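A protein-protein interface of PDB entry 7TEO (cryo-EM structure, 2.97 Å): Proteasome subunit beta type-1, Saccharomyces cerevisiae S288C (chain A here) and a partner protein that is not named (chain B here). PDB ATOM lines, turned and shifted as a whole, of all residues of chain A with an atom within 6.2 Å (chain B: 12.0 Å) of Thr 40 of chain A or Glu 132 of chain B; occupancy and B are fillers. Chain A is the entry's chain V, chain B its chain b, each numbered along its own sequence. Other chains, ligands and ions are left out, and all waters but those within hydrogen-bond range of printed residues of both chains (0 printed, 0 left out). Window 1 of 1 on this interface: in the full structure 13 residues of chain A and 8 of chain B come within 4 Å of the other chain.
OE1 of Glu 132 of chain B sits at hydrogen-bond distance from OG1 of Thr 20 of chain A (3.0 Å). The side-chain carboxylate of Asp 130 of chain B is in hydrogen-bond range of the side-chain hydroxyl of Ser 187 of chain A, 2.9 Å away. The side-chain hydroxyl of Thr 40 of chain A sits at hydrogen-bond distance from the backbone carbonyl oxygen of Asp 130 of chain B, 2.9 Å away. OD2 of Asp 130 of chain B sits at hydrogen-bond distance from N of Thr 20 of chain A. The side-chain carboxylate (OE2) of Glu 132 of chain B sits at hydrogen-bond distance from the backbone NH (N) of Thr 40 of chain A, at 3.2 Å. OG of Ser 67 of chain A sits at hydrogen-bond distance from OE1 of Gln 134 of chain B. OD2 of Asp 130 of chain B is in hydrogen-bond range of OG of Ser 148 of chain A, at 2.5 Å. The backbone NH (N) of Ala 68 of chain A lies within hydrogen-bond range of the backbone carbonyl oxygen (O) of Glu 132 of chain B, at 2.5 Å.
Tyr 133 of chain B touches Thr 39 of chain A (OH to CG2, 3.3 Å). CA of Asp 131 of chain B touches O of Thr 40 of chain A (3.6 Å). Thr 41 of chain A touches Tyr 133 of chain B (CG2 to CD2, 3.3 Å). Gln 136 of chain B touches Thr 41 of chain A. CB of Phe 129 of chain B touches O of Gly 42 of chain A (3.5 Å). N of Gly 42 of chain A touches O of Asp 130 of chain B, 3.5 Å away. Asn 47 of chain A touches Tyr 133 of chain B (CB to OH, 3.4 Å). Gly 66 of chain A touches Glu 132 of chain B. Glu 132 of chain B touches Ser 67 of chain A (O to C, 3.5 Å). Ala 69 of chain A touches Gln 134 of chain B (CB to OE1, 3.98 Å).
Of the 20 printed residues of chain A, 13 touch a printed residue of chain B. Printed residues of chain A that touch a printed residue of chain B: Thr 20, Thr 39, Thr 40, Thr 41, Gly 42, Ala 46, Asn 47, Gly 66, Ser 67, Ala 68, Ala 69, Ser 148 and Ser 187. Among the printed residues, no Asp or Glu carboxylate lies within 4 Å of a Lys or Arg side-chain nitrogen of the other chain.
Of chain B, only Asp 130 (2.8 Å) and Glu 132 (3.0 Å) come within 4 Å of Thr 20 of chain A. Thr 39 of chain A touches just these residues of chain B: Glu 132 and Tyr 133. Of chain B, only Asp 130 (2.8 Å), Asp 131 (3.6 Å) and Glu 132 (2.7 Å) come within 4 Å of Thr 40 of chain A. Of chain B, only Phe 129 and Asp 130 come within 4 Å of Gly 42 of chain A. No residue of chain B comes within 4 Å of Ala 43 of chain A. No residue of chain B comes within 4 Å of Ile 45 of chain A. Ala 46 of chain A touches one residue of chain B. Gly 66 of chain A touches just one residue of chain B: Glu 132 (3.9 Å). Of the printed residues of chain B, Ala 68 of chain A touches Glu 132 (2.5 Å). Of the printed residues of chain B, Ala 69 of chain A touches Gln 134. No residue of chain B comes within 4 Å of Gly 186 of chain A. Ser 187 of chain A touches just one residue of chain B: Asp 130 (2.9 Å). No residue of chain B comes within 4 Å of Ser 188 of chain A. Lys 128 of chain B touches none of the printed residues of chain A. Glu 132 of chain B touches just these residues of chain A: Thr 20, Thr 39, Thr 40, Gly 66, Ser 67 and Ala 68. Printed residues of chain A within 4 Å of Gln 134 of chain B: Ser 67 and Ala 69. Of the printed residues of chain A, Ala 135 of chain B touches Thr 41. The nearest residue of chain A that does not touch Glu 132 of chain B is Ala 69 of chain A (4.1 Å).
N of Thr 20 of chain A lies close to OG of Ser 188 of chain A. N of Thr 20 of chain A lies within hydrogen-bond range of OG of Ser 187 of chain A, at 3.3 Å. N of Thr 39 of chain A sits at hydrogen-bond distance from O of Asn 47 of chain A. N of Ala 69 of chain A sits close to OG of Ser 67 of chain A (3.5 Å). The side-chain hydroxyl (OG1) of Thr 20 of chain A sits at hydrogen-bond distance from the side-chain amino group (NZ) of Lys 52 of chain A. N of Gln 134 of chain B is in hydrogen-bond range of OD1 of Asp 131 of chain B.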
ATOM      1  N   THR A  20       6.057 -16.832  -0.775  1.00  0.00           N
ATOM      2  CA  THR A  20       6.507 -18.087  -0.111  1.00  0.00           C
ATOM      3  C   THR A  20       5.390 -18.661   0.749  1.00  0.00           C
ATOM      4  O   THR A  20       4.584 -17.918   1.306  1.00  0.00           O
ATOM      5  CB  THR A  20       7.749 -17.846   0.763  1.00  0.00           C
ATOM      6  OG1 THR A  20       8.835 -17.398  -0.057  1.00  0.00           O
ATOM      7  CG2 THR A  20       8.151 -19.118   1.480  1.00  0.00           C
ATOM      8  N   ARG A  38       8.746 -21.836  -5.470  1.00  0.00           N
ATOM      9  CA  ARG A  38       8.890 -20.616  -6.255  1.00  0.00           C
ATOM     10  C   ARG A  38       9.617 -19.536  -5.463  1.00  0.00           C
ATOM     11  O   ARG A  38       9.283 -19.271  -4.305  1.00  0.00           O
ATOM     12  CB  ARG A  38       7.524 -20.097  -6.702  1.00  0.00           C
ATOM     13  CG  ARG A  38       7.582 -18.757  -7.426  1.00  0.00           C
ATOM     14  CD  ARG A  38       6.212 -18.297  -7.883  1.00  0.00           C
ATOM     15  NE  ARG A  38       5.681 -19.138  -8.947  1.00  0.00           N
ATOM     16  CZ  ARG A  38       4.500 -18.965  -9.522  1.00  0.00           C
ATOM     17  NH1 ARG A  38       3.693 -17.980  -9.162  1.00  0.00           N
ATOM     18  NH2 ARG A  38       4.119 -19.799 -10.484  1.00  0.00           N
ATOM     19  N   THR A  39      10.609 -18.913  -6.097  1.00  0.00           N
ATOM     20  CA  THR A  39      11.266 -17.716  -5.590  1.00  0.00           C
ATOM     21  C   THR A  39      11.160 -16.617  -6.637  1.00  0.00           C
ATOM     22  O   THR A  39      11.379 -16.862  -7.826  1.00  0.00           O
ATOM     23  CB  THR A  39      12.737 -17.981  -5.259  1.00  0.00           C
ATOM     24  OG1 THR A  39      12.827 -18.964  -4.223  1.00  0.00           O
ATOM     25  CG2 THR A  39      13.425 -16.707  -4.800  1.00  0.00           C
ATOM     26  N   THR A  40      10.833 -15.405  -6.195  1.00  0.00           N
ATOM     27  CA  THR A  40      10.568 -14.295  -7.097  1.00  0.00           C
ATOM     28  C   THR A  40      11.378 -13.067  -6.704  1.00  0.00           C
ATOM     29  O   THR A  40      11.667 -12.838  -5.527  1.00  0.00           O
ATOM     30  CB  THR A  40       9.077 -13.927  -7.108  1.00  0.00           C
ATOM     31  OG1 THR A  40       8.693 -13.418  -5.825  1.00  0.00           O
ATOM     32  CG2 THR A  40       8.224 -15.138  -7.444  1.00  0.00           C
ATOM     33  N   THR A  41      11.735 -12.278  -7.715  1.00  0.00           N
ATOM     34  CA  THR A  41      12.338 -10.956  -7.551  1.00  0.00           C
ATOM     35  C   THR A  41      11.359  -9.975  -8.186  1.00  0.00           C
ATOM     36  O   THR A  41      11.440  -9.688  -9.382  1.00  0.00           O
ATOM     37  CB  THR A  41      13.715 -10.868  -8.202  1.00  0.00           C
ATOM     38  OG1 THR A  41      13.622 -11.262  -9.577  1.00  0.00           O
ATOM     39  CG2 THR A  41      14.703 -11.767  -7.486  1.00  0.00           C
ATOM     40  N   GLY A  42      10.438  -9.454  -7.381  1.00  0.00           N
ATOM     41  CA  GLY A  42       9.334  -8.705  -7.951  1.00  0.00           C
ATOM     42  C   GLY A  42       8.363  -9.647  -8.635  1.00  0.00           C
ATOM     43  O   GLY A  42       7.976 -10.684  -8.087  1.00  0.00           O
ATOM     44  N   ALA A  43       7.959  -9.288  -9.852  1.00  0.00           N
ATOM     45  CA  ALA A  43       7.046 -10.122 -10.622  1.00  0.00           C
ATOM     46  C   ALA A  43       7.750 -11.247 -11.369  1.00  0.00           C
ATOM     47  O   ALA A  43       7.071 -12.120 -11.920  1.00  0.00           O
ATOM     48  CB  ALA A  43       6.266  -9.262 -11.617  1.00  0.00           C
ATOM     49  N   TYR A  44       9.079 -11.248 -11.405  1.00  0.00           N
ATOM     50  CA  TYR A  44       9.826 -12.257 -12.143  1.00  0.00           C
ATOM     51  C   TYR A  44      10.131 -13.449 -11.245  1.00  0.00           C
ATOM     52  O   TYR A  44      10.599 -13.281 -10.116  1.00  0.00           O
ATOM     53  CB  TYR A  44      11.124 -11.657 -12.679  1.00  0.00           C
ATOM     54  CG  TYR A  44      12.035 -12.649 -13.360  1.00  0.00           C
ATOM     55  CD1 TYR A  44      11.580 -13.433 -14.408  1.00  0.00           C
ATOM     56  CD2 TYR A  44      13.353 -12.798 -12.955  1.00  0.00           C
ATOM     57  CE1 TYR A  44      12.412 -14.341 -15.030  1.00  0.00           C
ATOM     58  CE2 TYR A  44      14.189 -13.701 -13.572  1.00  0.00           C
ATOM     59  CZ  TYR A  44      13.715 -14.468 -14.609  1.00  0.00           C
ATOM     60  OH  TYR A  44      14.545 -15.370 -15.227  1.00  0.00           O
ATOM     61  N   ILE A  45       9.867 -14.653 -11.747  1.00  0.00           N
ATOM     62  CA  ILE A  45      10.186 -15.870 -11.012  1.00  0.00           C
ATOM     63  C   ILE A  45      11.650 -16.208 -11.253  1.00  0.00           C
ATOM     64  O   ILE A  45      11.989 -16.916 -12.207  1.00  0.00           O
ATOM     65  CB  ILE A  45       9.272 -17.038 -11.427  1.00  0.00           C
ATOM     66  CG1 ILE A  45       7.821 -16.724 -11.066  1.00  0.00           C
ATOM     67  CG2 ILE A  45       9.718 -18.326 -10.756  1.00  0.00           C
ATOM     68  CD1 ILE A  45       6.813 -17.583 -11.792  1.00  0.00           C
ATOM     69  N   ALA A  46      12.528 -15.706 -10.383  1.00  0.00           N
ATOM     70  CA  ALA A  46      13.959 -15.907 -10.565  1.00  0.00           C
ATOM     71  C   ALA A  46      14.370 -17.363 -10.394  1.00  0.00           C
ATOM     72  O   ALA A  46      15.399 -17.769 -10.940  1.00  0.00           O
ATOM     73  CB  ALA A  46      14.734 -15.030  -9.585  1.00  0.00           C
ATOM     74  N   ASN A  47      13.596 -18.150  -9.652  1.00  0.00           N
ATOM     75  CA  ASN A  47      13.888 -19.564  -9.463  1.00  0.00           C
ATOM     76  C   ASN A  47      12.589 -20.268  -9.110  1.00  0.00           C
ATOM     77  O   ASN A  47      11.955 -19.927  -8.109  1.00  0.00           O
ATOM     78  CB  ASN A  47      14.932 -19.775  -8.363  1.00  0.00           C
ATOM     79  CG  ASN A  47      15.469 -21.188  -8.333  1.00  0.00           C
ATOM     80  OD1 ASN A  47      14.992 -22.060  -9.058  1.00  0.00           O
ATOM     81  ND2 ASN A  47      16.469 -21.425  -7.495  1.00  0.00           N
ATOM     82  N   LYS A  52      13.360 -24.806  -0.201  1.00  0.00           N
ATOM     83  CA  LYS A  52      13.347 -23.902   0.941  1.00  0.00           C
ATOM     84  C   LYS A  52      13.518 -24.615   2.277  1.00  0.00           C
ATOM     85  O   LYS A  52      13.566 -23.943   3.312  1.00  0.00           O
ATOM     86  CB  LYS A  52      12.045 -23.102   0.940  1.00  0.00           C
ATOM     87  CG  LYS A  52      11.928 -22.160  -0.247  1.00  0.00           C
ATOM     88  CD  LYS A  52      10.612 -21.411  -0.257  1.00  0.00           C
ATOM     89  CE  LYS A  52      10.527 -20.482  -1.453  1.00  0.00           C
ATOM     90  NZ  LYS A  52       9.234 -19.756  -1.503  1.00  0.00           N
ATOM     91  N   GLY A  66      11.416 -14.697   4.403  1.00  0.00           N
ATOM     92  CA  GLY A  66      11.966 -13.356   4.431  1.00  0.00           C
ATOM     93  C   GLY A  66      13.175 -13.224   3.529  1.00  0.00           C
ATOM     94  O   GLY A  66      13.221 -13.831   2.456  1.00  0.00           O
ATOM     95  N   SER A  67      14.159 -12.431   3.947  1.00  0.00           N
ATOM     96  CA  SER A  67      15.350 -12.232   3.135  1.00  0.00           C
ATOM     97  C   SER A  67      16.103 -13.543   2.962  1.00  0.00           C
ATOM     98  O   SER A  67      16.376 -14.251   3.935  1.00  0.00           O
ATOM     99  CB  SER A  67      16.256 -11.186   3.784  1.00  0.00           C
ATOM    100  OG  SER A  67      17.543 -11.195   3.196  1.00  0.00           O
ATOM    101  N   ALA A  68      16.439 -13.870   1.711  1.00  0.00           N
ATOM    102  CA  ALA A  68      17.188 -15.095   1.450  1.00  0.00           C
ATOM    103  C   ALA A  68      18.598 -15.025   2.016  1.00  0.00           C
ATOM    104  O   ALA A  68      19.081 -16.006   2.593  1.00  0.00           O
ATOM    105  CB  ALA A  68      17.239 -15.373  -0.052  1.00  0.00           C
ATOM    106  N   ALA A  69      19.273 -13.885   1.864  1.00  0.00           N
ATOM    107  CA  ALA A  69      20.634 -13.765   2.373  1.00  0.00           C
ATOM    108  C   ALA A  69      20.670 -13.902   3.889  1.00  0.00           C
ATOM    109  O   ALA A  69      21.505 -14.637   4.433  1.00  0.00           O
ATOM    110  CB  ALA A  69      21.235 -12.428   1.946  1.00  0.00           C
ATOM    111  N   SER A 148       4.476 -15.328   2.638  1.00  0.00           N
ATOM    112  CA  SER A 148       3.458 -14.426   2.115  1.00  0.00           C
ATOM    113  C   SER A 148       2.164 -15.150   1.773  1.00  0.00           C
ATOM    114  O   SER A 148       1.095 -14.532   1.797  1.00  0.00           O
ATOM    115  CB  SER A 148       3.988 -13.707   0.874  1.00  0.00           C
ATOM    116  OG  SER A 148       4.422 -14.637  -0.101  1.00  0.00           O
ATOM    117  N   GLY A 186       0.655 -14.962  -5.611  1.00  0.00           N
ATOM    118  CA  GLY A 186       1.481 -14.926  -6.804  1.00  0.00           C
ATOM    119  C   GLY A 186       2.940 -15.215  -6.520  1.00  0.00           C
ATOM    120  O   GLY A 186       3.676 -15.649  -7.410  1.00  0.00           O
ATOM    121  N   SER A 187       3.381 -14.980  -5.286  1.00  0.00           N
ATOM    122  CA  SER A 187       4.757 -15.246  -4.888  1.00  0.00           C
ATOM    123  C   SER A 187       4.996 -16.695  -4.484  1.00  0.00           C
ATOM    124  O   SER A 187       6.139 -17.051  -4.182  1.00  0.00           O
ATOM    125  CB  SER A 187       5.151 -14.321  -3.734  1.00  0.00           C
ATOM    126  OG  SER A 187       4.375 -14.588  -2.579  1.00  0.00           O
ATOM    127  N   SER A 188       3.961 -17.532  -4.466  1.00  0.00           N
ATOM    128  CA  SER A 188       4.088 -18.945  -4.141  1.00  0.00           C
ATOM    129  C   SER A 188       3.705 -19.776  -5.354  1.00  0.00           C
ATOM    130  O   SER A 188       2.791 -19.413  -6.101  1.00  0.00           O
ATOM    131  CB  SER A 188       3.197 -19.330  -2.957  1.00  0.00           C
ATOM    132  OG  SER A 188       3.724 -18.845  -1.736  1.00  0.00           O
ATOM    133  N   PRO B 127      -0.843  -5.586  -1.351  1.00  0.00           N
ATOM    134  CA  PRO B 127      -0.016  -6.792  -1.230  1.00  0.00           C
ATOM    135  C   PRO B 127       1.212  -6.758  -2.136  1.00  0.00           C
ATOM    136  O   PRO B 127       1.081  -6.782  -3.358  1.00  0.00           O
ATOM    137  CB  PRO B 127      -0.976  -7.914  -1.643  1.00  0.00           C
ATOM    138  CG  PRO B 127      -2.329  -7.369  -1.351  1.00  0.00           C
ATOM    139  CD  PRO B 127      -2.237  -5.915  -1.689  1.00  0.00           C
ATOM    140  N   LYS B 128       2.396  -6.702  -1.531  1.00  0.00           N
ATOM    141  CA  LYS B 128       3.634  -6.602  -2.286  1.00  0.00           C
ATOM    142  C   LYS B 128       4.171  -7.987  -2.638  1.00  0.00           C
ATOM    143  O   LYS B 128       3.864  -8.990  -1.986  1.00  0.00           O
ATOM    144  CB  LYS B 128       4.683  -5.825  -1.489  1.00  0.00           C
ATOM    145  CG  LYS B 128       4.669  -4.322  -1.732  1.00  0.00           C
ATOM    146  CD  LYS B 128       3.462  -3.643  -1.095  1.00  0.00           C
ATOM    147  CE  LYS B 128       3.534  -3.669   0.426  1.00  0.00           C
ATOM    148  NZ  LYS B 128       2.543  -2.751   1.053  1.00  0.00           N
ATOM    149  N   PHE B 129       4.988  -8.031  -3.687  1.00  0.00           N
ATOM    150  CA  PHE B 129       5.639  -9.266  -4.094  1.00  0.00           C
ATOM    151  C   PHE B 129       6.865  -9.541  -3.229  1.00  0.00           C
ATOM    152  O   PHE B 129       7.492  -8.630  -2.683  1.00  0.00           O
ATOM    153  CB  PHE B 129       6.057  -9.204  -5.563  1.00  0.00           C
ATOM    154  CG  PHE B 129       4.953  -9.535  -6.527  1.00  0.00           C
ATOM    155  CD1 PHE B 129       4.693 -10.847  -6.877  1.00  0.00           C
ATOM    156  CD2 PHE B 129       4.185  -8.532  -7.094  1.00  0.00           C
ATOM    157  CE1 PHE B 129       3.684 -11.156  -7.763  1.00  0.00           C
ATOM    158  CE2 PHE B 129       3.175  -8.838  -7.983  1.00  0.00           C
ATOM    159  CZ  PHE B 129       2.926 -10.153  -8.318  1.00  0.00           C
ATOM    160  N   ASP B 130       7.200 -10.823  -3.111  1.00  0.00           N
ATOM    161  CA  ASP B 130       8.389 -11.215  -2.369  1.00  0.00           C
ATOM    162  C   ASP B 130       9.645 -10.918  -3.177  1.00  0.00           C
ATOM    163  O   ASP B 130       9.691 -11.133  -4.391  1.00  0.00           O
ATOM    164  CB  ASP B 130       8.334 -12.704  -2.024  1.00  0.00           C
ATOM    165  CG  ASP B 130       7.304 -13.018  -0.958  1.00  0.00           C
ATOM    166  OD1 ASP B 130       7.044 -12.145  -0.105  1.00  0.00           O
ATOM    167  OD2 ASP B 130       6.758 -14.142  -0.970  1.00  0.00           O
ATOM    168  N   ASP B 131      10.674 -10.418  -2.491  1.00  0.00           N
ATOM    169  CA  ASP B 131      12.009 -10.234  -3.066  1.00  0.00           C
ATOM    170  C   ASP B 131      12.972 -10.934  -2.113  1.00  0.00           C
ATOM    171  O   ASP B 131      13.568 -10.309  -1.234  1.00  0.00           O
ATOM    172  CB  ASP B 131      12.343  -8.754  -3.247  1.00  0.00           C
ATOM    173  CG  ASP B 131      13.681  -8.535  -3.930  1.00  0.00           C
ATOM    174  OD1 ASP B 131      14.552  -9.425  -3.846  1.00  0.00           O
ATOM    175  OD2 ASP B 131      13.861  -7.469  -4.555  1.00  0.00           O
ATOM    176  N   GLU B 132      13.122 -12.247  -2.298  1.00  0.00           N
ATOM    177  CA  GLU B 132      13.918 -13.038  -1.367  1.00  0.00           C
ATOM    178  C   GLU B 132      15.399 -12.703  -1.477  1.00  0.00           C
ATOM    179  O   GLU B 132      16.107 -12.663  -0.464  1.00  0.00           O
ATOM    180  CB  GLU B 132      13.677 -14.525  -1.622  1.00  0.00           C
ATOM    181  CG  GLU B 132      12.322 -15.018  -1.137  1.00  0.00           C
ATOM    182  CD  GLU B 132      11.268 -15.007  -2.228  1.00  0.00           C
ATOM    183  OE1 GLU B 132      10.197 -15.619  -2.028  1.00  0.00           O
ATOM    184  OE2 GLU B 132      11.505 -14.381  -3.281  1.00  0.00           O
ATOM    185  N   TYR B 133      15.886 -12.456  -2.692  1.00  0.00           N
ATOM    186  CA  TYR B 133      17.296 -12.144  -2.887  1.00  0.00           C
ATOM    187  C   TYR B 133      17.626 -10.694  -2.573  1.00  0.00           C
ATOM    188  O   TYR B 133      18.807 -10.331  -2.603  1.00  0.00           O
ATOM    189  CB  TYR B 133      17.708 -12.436  -4.327  1.00  0.00           C
ATOM    190  CG  TYR B 133      17.340 -13.818  -4.801  1.00  0.00           C
ATOM    191  CD1 TYR B 133      17.674 -14.945  -4.063  1.00  0.00           C
ATOM    192  CD2 TYR B 133      16.661 -13.994  -5.995  1.00  0.00           C
ATOM    193  CE1 TYR B 133      17.331 -16.206  -4.504  1.00  0.00           C
ATOM    194  CE2 TYR B 133      16.319 -15.246  -6.443  1.00  0.00           C
ATOM    195  CZ  TYR B 133      16.653 -16.349  -5.696  1.00  0.00           C
ATOM    196  OH  TYR B 133      16.309 -17.601  -6.149  1.00  0.00           O
ATOM    197  N   GLN B 134      16.627  -9.862  -2.284  1.00  0.00           N
ATOM    198  CA  GLN B 134      16.813  -8.422  -2.141  1.00  0.00           C
ATOM    199  C   GLN B 134      17.321  -7.790  -3.431  1.00  0.00           C
ATOM    200  O   GLN B 134      17.963  -6.736  -3.400  1.00  0.00           O
ATOM    201  CB  GLN B 134      17.764  -8.102  -0.984  1.00  0.00           C
ATOM    202  CG  GLN B 134      17.499  -8.912   0.273  1.00  0.00           C
ATOM    203  CD  GLN B 134      18.251  -8.384   1.476  1.00  0.00           C
ATOM    204  OE1 GLN B 134      19.186  -9.018   1.964  1.00  0.00           O
ATOM    205  NE2 GLN B 134      17.846  -7.217   1.963  1.00  0.00           N
ATOM    206  N   ALA B 135      17.037  -8.425  -4.572  1.00  0.00           N
ATOM    207  CA  ALA B 135      17.539  -7.929  -5.847  1.00  0.00           C
ATOM    208  C   ALA B 135      17.019  -6.533  -6.156  1.00  0.00           C
ATOM    209  O   ALA B 135      17.770  -5.688  -6.658  1.00  0.00           O
ATOM    210  CB  ALA B 135      17.151  -8.891  -6.968  1.00  0.00           C
ATOM    211  N   GLN B 136      15.747  -6.267  -5.866  1.00  0.00           N
ATOM    212  CA  GLN B 136      15.155  -4.959  -6.105  1.00  0.00           C
ATOM    213  C   GLN B 136      15.273  -4.045  -4.894  1.00  0.00           C
ATOM    214  O   GLN B 136      14.747  -2.927  -4.922  1.00  0.00           O
ATOM    215  CB  GLN B 136      13.686  -5.106  -6.504  1.00  0.00           C
ATOM    216  CG  GLN B 136      13.457  -6.010  -7.703  1.00  0.00           C
ATOM    217  CD  GLN B 136      12.224  -5.628  -8.495  1.00  0.00           C
ATOM    218  OE1 GLN B 136      11.360  -4.901  -8.008  1.00  0.00           O
ATOM    219  NE2 GLN B 136      12.136  -6.121  -9.725  1.00  0.00           N
ATOM    220  N   ALA B 137      15.943  -4.492  -3.836  1.00  0.00           N
ATOM    221  CA  ALA B 137      16.174  -3.631  -2.686  1.00  0.00           C
ATOM    222  C   ALA B 137      16.996  -2.423  -3.110  1.00  0.00           C
ATOM    223  O   ALA B 137      18.025  -2.563  -3.779  1.00  0.00           O
ATOM    224  CB  ALA B 137      16.890  -4.403  -1.579  1.00  0.00           C
ATOM    225  N   ARG B 138      16.542  -1.237  -2.719  1.00  0.00           N
ATOM    226  CA  ARG B 138      17.172   0.014  -3.106  1.00  0.00           C
ATOM    227  C   ARG B 138      17.767   0.690  -1.878  1.00  0.00           C
ATOM    228  O   ARG B 138      17.199   0.638  -0.783  1.00  0.00           O
ATOM    229  CB  ARG B 138      16.169   0.955  -3.784  1.00  0.00           C
ATOM    230  CG  ARG B 138      15.300   0.288  -4.844  1.00  0.00           C
ATOM    231  CD  ARG B 138      16.129  -0.355  -5.946  1.00  0.00           C
ATOM    232  NE  ARG B 138      15.290  -0.990  -6.955  1.00  0.00           N
ATOM    233  CZ  ARG B 138      15.751  -1.675  -7.993  1.00  0.00           C
ATOM    234  NH1 ARG B 138      17.048  -1.831  -8.198  1.00  0.00           N
ATOM    235  NH2 ARG B 138      14.888  -2.218  -8.847  1.00  0.00           N
ATOM    236  N   PHE B 227      19.464  -8.228 -13.170  1.00  0.00           N
ATOM    237  CA  PHE B 227      18.294  -9.020 -13.515  1.00  0.00           C
ATOM    238  C   PHE B 227      17.497  -8.458 -14.681  1.00  0.00           C
ATOM    239  O   PHE B 227      16.516  -9.086 -15.094  1.00  0.00           O
ATOM    240  CB  PHE B 227      17.369  -9.146 -12.296  1.00  0.00           C
ATOM    241  CG  PHE B 227      17.896 -10.059 -11.228  1.00  0.00           C
ATOM    242  CD1 PHE B 227      17.727 -11.430 -11.320  1.00  0.00           C
ATOM    243  CD2 PHE B 227      18.564  -9.542 -10.132  1.00  0.00           C
ATOM    244  CE1 PHE B 227      18.216 -12.268 -10.335  1.00  0.00           C
ATOM    245  CE2 PHE B 227      19.053 -10.374  -9.147  1.00  0.00           C
ATOM    246  CZ  PHE B 227      18.879 -11.737  -9.247  1.00  0.00           C
ATOM    247  N   GLY B 228      17.878  -7.305 -15.221  1.00  0.00           N
ATOM    248  CA  GLY B 228      17.115  -6.681 -16.272  1.00  0.00           C
ATOM    249  C   GLY B 228      15.851  -6.045 -15.731  1.00  0.00           C
ATOM    250  O   GLY B 228      15.685  -5.879 -14.518  1.00  0.00           O
ATOM    251  N   PRO B 229      14.927  -5.672 -16.625  1.00  0.00           N
ATOM    252  CA  PRO B 229      13.668  -5.042 -16.214  1.00  0.00           C
ATOM    253  C   PRO B 229      12.667  -6.038 -15.637  1.00  0.00           C
ATOM    254  O   PRO B 229      11.630  -5.616 -15.126  1.00  0.00           O
ATOM    255  CB  PRO B 229      13.146  -4.435 -17.517  1.00  0.00           C
ATOM    256  CG  PRO B 229      13.703  -5.310 -18.580  1.00  0.00           C
ATOM    257  CD  PRO B 229      15.049  -5.756 -18.091  1.00  0.00           C
